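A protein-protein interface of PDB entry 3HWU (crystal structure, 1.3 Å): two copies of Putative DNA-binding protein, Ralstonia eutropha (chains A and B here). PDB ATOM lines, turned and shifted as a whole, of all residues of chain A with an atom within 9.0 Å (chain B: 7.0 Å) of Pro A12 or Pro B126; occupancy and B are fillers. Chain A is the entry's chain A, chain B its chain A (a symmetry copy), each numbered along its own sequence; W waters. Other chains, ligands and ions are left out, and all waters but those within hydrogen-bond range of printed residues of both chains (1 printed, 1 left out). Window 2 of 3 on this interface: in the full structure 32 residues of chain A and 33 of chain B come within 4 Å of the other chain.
The side-chain sulfur of Met A9 lies close to the side-chain amide nitrogen of Gln B127, 3.7 Å away.
The backbone carbonyl oxygen of Lys A10 lies within hydrogen-bond range of the side-chain amide nitrogen of Gln B127 (3.0 Å).
The backbone carbonyl oxygen (O) of Ser B40 is in hydrogen-bond range of the backbone NH (N) of Tyr B125.
OG1 of Thr A11 lies within hydrogen-bond range of N of Tyr A15 (3.3 Å).
The backbone NH (N) of Met A9 lies within hydrogen-bond range of the backbone carbonyl oxygen (O) of Leu A16.
The backbone NH (N) of Gly A14 is in hydrogen-bond range of the side-chain hydroxyl (OG1) of Thr A11 (3.0 Å).
OG of Ser B40 lies within hydrogen-bond range of O of Gln B127 (2.8 Å).
O of Thr A13 is in hydrogen-bond range of N of Val A124 (3.0 Å).
Among the printed residues, pairs that only touch across the chains: Thr A11 with Tyr B125 (3.5 Å), Thr A13 with Thr B13 (3.8 Å), Pro A12 with Pro B126 (3.8 Å), Met A9 with Tyr B125 (3.9 Å) and Leu A16 with Leu B129 (3.98 Å).
Of the printed residues of chain B, Met A9 touches Tyr B125 and Gln B127.
Printed residues of chain B within 4 Å of Pro A12: Pro B126.
Of the printed residues of chain B, Thr A13 touches Thr B13.
Gly A14 touches none of the printed residues of chain B.
Of the printed residues of chain A, Thr B13 touches Thr A13.
Ser B40 touches none of the printed residues of chain A.
Of the printed residues of chain A, Tyr B125 touches Met A9 and Thr A11.
Pro B126 touches just one residue of chain A: Pro A12 (3.8 Å).
The nearest printed residue of chain B that does not touch Lys A10 is Pro B126 (5.9 Å).
Printed residues of chain B that touch a printed residue of chain A: Thr B13, Tyr B125, Pro B126, Gln B127 and Leu B129.
Thr B13 touches its own counterpart, Thr A13.
Of the 7 pairs that touch across the chains among the printed residues, 1 has its exchanged pair printed and touching as well.
Water W1 lies within hydrogen-bond range of OG1 of Thr A11, O of Tyr A15, OH of Tyr B125 and O of Val A122.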
ATOM      1  N   MET A   9      20.987 -25.597 -21.273  1.00  0.00           N
ATOM      2  CA  MET A   9      20.784 -26.926 -21.845  1.00  0.00           C
ATOM      3  C   MET A   9      19.985 -26.812 -23.136  1.00  0.00           C
ATOM      4  O   MET A   9      19.136 -25.934 -23.281  1.00  0.00           O
ATOM      5  CB  MET A   9      20.094 -27.895 -20.868  1.00  0.00           C
ATOM      6  CG  MET A   9      18.614 -27.750 -20.696  1.00  0.00           C
ATOM      7  SD  MET A   9      17.932 -28.998 -19.349  1.00  0.00           S
ATOM      8  CE  MET A   9      16.141 -28.718 -19.905  1.00  0.00           C
ATOM      9  N   LYS A  10      20.269 -27.701 -24.069  1.00  0.00           N
ATOM     10  CA  LYS A  10      19.481 -27.811 -25.296  1.00  0.00           C
ATOM     11  C   LYS A  10      18.144 -28.466 -24.993  1.00  0.00           C
ATOM     12  O   LYS A  10      18.099 -29.497 -24.305  1.00  0.00           O
ATOM     13  CB  LYS A  10      20.265 -28.606 -26.380  1.00  0.00           C
ATOM     14  CG  LYS A  10      19.656 -28.513 -27.797  1.00  0.00           C
ATOM     15  CD  LYS A  10      20.197 -29.496 -28.820  1.00  0.00           C
ATOM     16  CE  LYS A  10      19.285 -29.511 -30.127  1.00  0.00           C
ATOM     17  NZ  LYS A  10      17.698 -29.631 -30.004  1.00  0.00           N
ATOM     18  N   THR A  11      17.085 -27.862 -25.537  1.00  0.00           N
ATOM     19  CA  THR A  11      15.732 -28.409 -25.441  1.00  0.00           C
ATOM     20  C   THR A  11      15.222 -28.724 -26.853  1.00  0.00           C
ATOM     21  O   THR A  11      15.785 -28.246 -27.844  1.00  0.00           O
ATOM     22  CB  THR A  11      14.786 -27.431 -24.761  1.00  0.00           C
ATOM     23  OG1 THR A  11      14.689 -26.284 -25.597  1.00  0.00           O
ATOM     24  CG2 THR A  11      15.301 -27.034 -23.363  1.00  0.00           C
ATOM     25  N   PRO A  12      14.109 -29.457 -26.963  1.00  0.00           N
ATOM     26  CA  PRO A  12      13.599 -29.741 -28.312  1.00  0.00           C
ATOM     27  C   PRO A  12      13.325 -28.512 -29.165  1.00  0.00           C
ATOM     28  O   PRO A  12      13.519 -28.543 -30.386  1.00  0.00           O
ATOM     29  CB  PRO A  12      12.348 -30.572 -28.051  1.00  0.00           C
ATOM     30  CG  PRO A  12      12.667 -31.319 -26.766  1.00  0.00           C
ATOM     31  CD  PRO A  12      13.433 -30.279 -25.933  1.00  0.00           C
ATOM     32  N   THR A  13      12.872 -27.434 -28.537  1.00  0.00           N
ATOM     33  CA  THR A  13      12.514 -26.227 -29.249  1.00  0.00           C
ATOM     34  C   THR A  13      13.556 -25.111 -29.192  1.00  0.00           C
ATOM     35  O   THR A  13      13.365 -24.075 -29.812  1.00  0.00           O
ATOM     36  CB  THR A  13      11.172 -25.698 -28.723  1.00  0.00           C
ATOM     37  OG1 THR A  13      11.282 -25.440 -27.331  1.00  0.00           O
ATOM     38  CG2 THR A  13      10.019 -26.709 -28.979  1.00  0.00           C
ATOM     39  N   GLY A  14      14.655 -25.312 -28.460  1.00  0.00           N
ATOM     40  CA  GLY A  14      15.638 -24.257 -28.347  1.00  0.00           C
ATOM     41  C   GLY A  14      16.596 -24.531 -27.194  1.00  0.00           C
ATOM     42  O   GLY A  14      17.365 -25.513 -27.250  1.00  0.00           O
ATOM     43  N   TYR A  15      16.586 -23.672 -26.171  1.00  0.00           N
ATOM     44  CA  TYR A  15      17.453 -23.828 -25.006  1.00  0.00           C
ATOM     45  C   TYR A  15      16.691 -23.412 -23.763  1.00  0.00           C
ATOM     46  O   TYR A  15      15.726 -22.628 -23.833  1.00  0.00           O
ATOM     47  CB  TYR A  15      18.692 -22.900 -25.120  1.00  0.00           C
ATOM     48  CG  TYR A  15      19.533 -23.231 -26.314  1.00  0.00           C
ATOM     49  CD1 TYR A  15      20.429 -24.294 -26.295  1.00  0.00           C
ATOM     50  CD2 TYR A  15      19.412 -22.513 -27.485  1.00  0.00           C
ATOM     51  CE1 TYR A  15      21.191 -24.611 -27.438  1.00  0.00           C
ATOM     52  CE2 TYR A  15      20.169 -22.828 -28.613  1.00  0.00           C
ATOM     53  CZ  TYR A  15      21.019 -23.876 -28.585  1.00  0.00           C
ATOM     54  OH  TYR A  15      21.717 -24.199 -29.735  1.00  0.00           O
ATOM     55  N   LEU A  16      17.152 -23.890 -22.616  1.00  0.00           N
ATOM     56  CA  LEU A  16      16.747 -23.373 -21.304  1.00  0.00           C
ATOM     57  C   LEU A  16      18.030 -22.888 -20.645  1.00  0.00           C
ATOM     58  O   LEU A  16      19.009 -23.642 -20.533  1.00  0.00           O
ATOM     59  CB  LEU A  16      16.133 -24.488 -20.437  1.00  0.00           C
ATOM     60  CG  LEU A  16      15.710 -24.077 -19.030  1.00  0.00           C
ATOM     61  CD1 LEU A  16      14.543 -23.063 -19.009  1.00  0.00           C
ATOM     62  CD2 LEU A  16      15.374 -25.319 -18.176  1.00  0.00           C
ATOM     63  N   VAL A 122      14.192 -20.256 -24.307  1.00  0.00           N
ATOM     64  CA  VAL A 122      14.555 -19.710 -25.607  1.00  0.00           C
ATOM     65  C   VAL A 122      14.026 -20.649 -26.701  1.00  0.00           C
ATOM     66  O   VAL A 122      14.298 -21.873 -26.684  1.00  0.00           O
ATOM     67  CB  VAL A 122      16.086 -19.587 -25.739  1.00  0.00           C
ATOM     68  CG1 VAL A 122      16.468 -18.951 -27.105  1.00  0.00           C
ATOM     69  CG2 VAL A 122      16.710 -18.772 -24.588  1.00  0.00           C
ATOM     70  N   THR A 123      13.232 -20.113 -27.616  1.00  0.00           N
ATOM     71  CA  THR A 123      12.688 -20.850 -28.768  1.00  0.00           C
ATOM     72  C   THR A 123      13.467 -20.404 -30.006  1.00  0.00           C
ATOM     73  O   THR A 123      13.418 -19.238 -30.375  1.00  0.00           O
ATOM     74  CB  THR A 123      11.218 -20.560 -28.944  1.00  0.00           C
ATOM     75  OG1 THR A 123      10.548 -20.869 -27.712  1.00  0.00           O
ATOM     76  CG2 THR A 123      10.605 -21.372 -30.071  1.00  0.00           C
ATOM     77  N   VAL A 124      14.208 -21.328 -30.636  1.00  0.00           N
ATOM     78  CA  VAL A 124      15.141 -21.018 -31.713  1.00  0.00           C
ATOM     79  C   VAL A 124      14.541 -21.300 -33.073  1.00  0.00           C
ATOM     80  O   VAL A 124      13.920 -22.334 -33.288  1.00  0.00           O
ATOM     81  CB  VAL A 124      16.438 -21.835 -31.547  1.00  0.00           C
ATOM     82  CG1 VAL A 124      17.415 -21.624 -32.718  1.00  0.00           C
ATOM     83  CG2 VAL A 124      17.148 -21.432 -30.241  1.00  0.00           C
ATOM     84  N   THR B  13       4.466 -29.590 -28.233  1.00  0.00           N
ATOM     85  CA  THR B  13       5.573 -29.173 -27.401  1.00  0.00           C
ATOM     86  C   THR B  13       5.373 -29.396 -25.902  1.00  0.00           C
ATOM     87  O   THR B  13       6.279 -29.126 -25.126  1.00  0.00           O
ATOM     88  CB  THR B  13       5.882 -27.692 -27.659  1.00  0.00           C
ATOM     89  OG1 THR B  13       4.727 -26.915 -27.377  1.00  0.00           O
ATOM     90  CG2 THR B  13       6.330 -27.448 -29.128  1.00  0.00           C
ATOM     91  N   ILE B  38       6.230 -35.271 -15.676  1.00  0.00           N
ATOM     92  CA  ILE B  38       6.971 -34.241 -16.389  1.00  0.00           C
ATOM     93  C   ILE B  38       8.394 -34.194 -15.891  1.00  0.00           C
ATOM     94  O   ILE B  38       8.618 -33.953 -14.687  1.00  0.00           O
ATOM     95  CB  ILE B  38       6.274 -32.853 -16.219  1.00  0.00           C
ATOM     96  CG1 ILE B  38       4.954 -32.879 -16.975  1.00  0.00           C
ATOM     97  CG2 ILE B  38       7.196 -31.738 -16.738  1.00  0.00           C
ATOM     98  CD1 ILE B  38       4.074 -31.598 -16.871  1.00  0.00           C
ATOM     99  N   PRO B  39       9.391 -34.381 -16.790  1.00  0.00           N
ATOM    100  CA  PRO B  39      10.777 -34.307 -16.271  1.00  0.00           C
ATOM    101  C   PRO B  39      11.156 -32.891 -15.799  1.00  0.00           C
ATOM    102  O   PRO B  39      11.695 -32.699 -14.721  1.00  0.00           O
ATOM    103  CB  PRO B  39      11.619 -34.835 -17.431  1.00  0.00           C
ATOM    104  CG  PRO B  39      10.639 -35.684 -18.252  1.00  0.00           C
ATOM    105  CD  PRO B  39       9.363 -34.880 -18.172  1.00  0.00           C
ATOM    106  N   SER B  40      10.852 -31.907 -16.641  1.00  0.00           N
ATOM    107  CA  SER B  40      10.935 -30.496 -16.342  1.00  0.00           C
ATOM    108  C   SER B  40      10.127 -29.760 -17.417  1.00  0.00           C
ATOM    109  O   SER B  40       9.804 -30.331 -18.457  1.00  0.00           O
ATOM    110  CB  SER B  40      12.383 -30.012 -16.326  1.00  0.00           C
ATOM    111  OG  SER B  40      13.052 -30.204 -17.580  1.00  0.00           O
ATOM    112  N   THR B 123       5.607 -26.095 -21.825  1.00  0.00           N
ATOM    113  CA  THR B 123       6.618 -26.645 -22.743  1.00  0.00           C
ATOM    114  C   THR B 123       7.442 -27.666 -21.958  1.00  0.00           C
ATOM    115  O   THR B 123       8.107 -27.308 -20.996  1.00  0.00           O
ATOM    116  CB  THR B 123       7.510 -25.551 -23.275  1.00  0.00           C
ATOM    117  OG1 THR B 123       6.681 -24.551 -23.887  1.00  0.00           O
ATOM    118  CG2 THR B 123       8.509 -26.073 -24.294  1.00  0.00           C
ATOM    119  N   VAL B 124       7.379 -28.946 -22.353  1.00  0.00           N
ATOM    120  CA  VAL B 124       7.959 -30.054 -21.601  1.00  0.00           C
ATOM    121  C   VAL B 124       9.300 -30.471 -22.163  1.00  0.00           C
ATOM    122  O   VAL B 124       9.467 -30.600 -23.370  1.00  0.00           O
ATOM    123  CB  VAL B 124       7.001 -31.263 -21.607  1.00  0.00           C
ATOM    124  CG1 VAL B 124       7.614 -32.495 -20.917  1.00  0.00           C
ATOM    125  CG2 VAL B 124       5.692 -30.899 -20.885  1.00  0.00           C
ATOM    126  N   TYR B 125      10.266 -30.658 -21.277  1.00  0.00           N
ATOM    127  CA  TYR B 125      11.627 -31.076 -21.653  1.00  0.00           C
ATOM    128  C   TYR B 125      11.870 -32.506 -21.215  1.00  0.00           C
ATOM    129  O   TYR B 125      11.292 -32.984 -20.237  1.00  0.00           O
ATOM    130  CB  TYR B 125      12.653 -30.178 -20.962  1.00  0.00           C
ATOM    131  CG  TYR B 125      12.354 -28.701 -21.160  1.00  0.00           C
ATOM    132  CD1 TYR B 125      12.079 -28.184 -22.430  1.00  0.00           C
ATOM    133  CD2 TYR B 125      12.328 -27.830 -20.084  1.00  0.00           C
ATOM    134  CE1 TYR B 125      11.779 -26.878 -22.609  1.00  0.00           C
ATOM    135  CE2 TYR B 125      12.058 -26.479 -20.287  1.00  0.00           C
ATOM    136  CZ  TYR B 125      11.809 -26.019 -21.559  1.00  0.00           C
ATOM    137  OH  TYR B 125      11.538 -24.677 -21.766  1.00  0.00           O
ATOM    138  N   PRO B 126      12.786 -33.207 -21.889  1.00  0.00           N
ATOM    139  CA  PRO B 126      13.042 -34.613 -21.523  1.00  0.00           C
ATOM    140  C   PRO B 126      13.896 -34.846 -20.290  1.00  0.00           C
ATOM    141  O   PRO B 126      13.869 -35.951 -19.742  1.00  0.00           O
ATOM    142  CB  PRO B 126      13.730 -35.179 -22.783  1.00  0.00           C
ATOM    143  CG  PRO B 126      14.391 -34.011 -23.396  1.00  0.00           C
ATOM    144  CD  PRO B 126      13.434 -32.839 -23.148  1.00  0.00           C
ATOM    145  N   GLN B 127      14.610 -33.820 -19.857  1.00  0.00           N
ATOM    146  CA  GLN B 127      15.535 -33.918 -18.733  1.00  0.00           C
ATOM    147  C   GLN B 127      14.851 -33.725 -17.385  1.00  0.00           C
ATOM    148  O   GLN B 127      14.182 -32.728 -17.152  1.00  0.00           O
ATOM    149  CB  GLN B 127      16.625 -32.841 -18.866  1.00  0.00           C
ATOM    150  CG  GLN B 127      17.437 -32.857 -20.172  1.00  0.00           C
ATOM    151  CD  GLN B 127      16.921 -31.921 -21.229  1.00  0.00           C
ATOM    152  OE1 GLN B 127      15.733 -31.636 -21.300  1.00  0.00           O
ATOM    153  NE2 GLN B 127      17.830 -31.434 -22.086  1.00  0.00           N
ATOM    154  N   ARG B 128      15.035 -34.679 -16.470  1.00  0.00           N
ATOM    155  CA  ARG B 128      14.557 -34.575 -15.112  1.00  0.00           C
ATOM    156  C   ARG B 128      15.446 -33.590 -14.365  1.00  0.00           C
ATOM    157  O   ARG B 128      16.652 -33.842 -14.198  1.00  0.00           O
ATOM    158  CB  ARG B 128      14.537 -35.979 -14.451  1.00  0.00           C
ATOM    159  CG  ARG B 128      14.210 -36.044 -12.948  1.00  0.00           C
ATOM    160  CD  ARG B 128      12.765 -35.917 -12.616  1.00  0.00           C
ATOM    161  NE  ARG B 128      12.712 -36.033 -11.149  1.00  0.00           N
ATOM    162  CZ  ARG B 128      11.649 -36.353 -10.451  1.00  0.00           C
ATOM    163  NH1 ARG B 128      10.526 -36.646 -11.042  1.00  0.00           N
ATOM    164  NH2 ARG B 128      11.742 -36.406  -9.114  1.00  0.00           N
ATOM    165  N   LEU B 129      14.858 -32.486 -13.877  1.00  0.00           N
ATOM    166  CA  LEU B 129      15.630 -31.452 -13.201  1.00  0.00           C
ATOM    167  C   LEU B 129      15.192 -31.286 -11.754  1.00  0.00           C
ATOM    168  O   LEU B 129      13.994 -31.285 -11.455  1.00  0.00           O
ATOM    169  CB  LEU B 129      15.509 -30.106 -13.922  1.00  0.00           C
ATOM    170  CG  LEU B 129      15.913 -30.011 -15.381  1.00  0.00           C
ATOM    171  CD1 LEU B 129      15.720 -28.543 -15.876  1.00  0.00           C
ATOM    172  CD2 LEU B 129      17.313 -30.550 -15.612  1.00  0.00           C
HETATM  173  O   HOH W   1      13.159 -24.138 -24.509  1.00  0.00           O
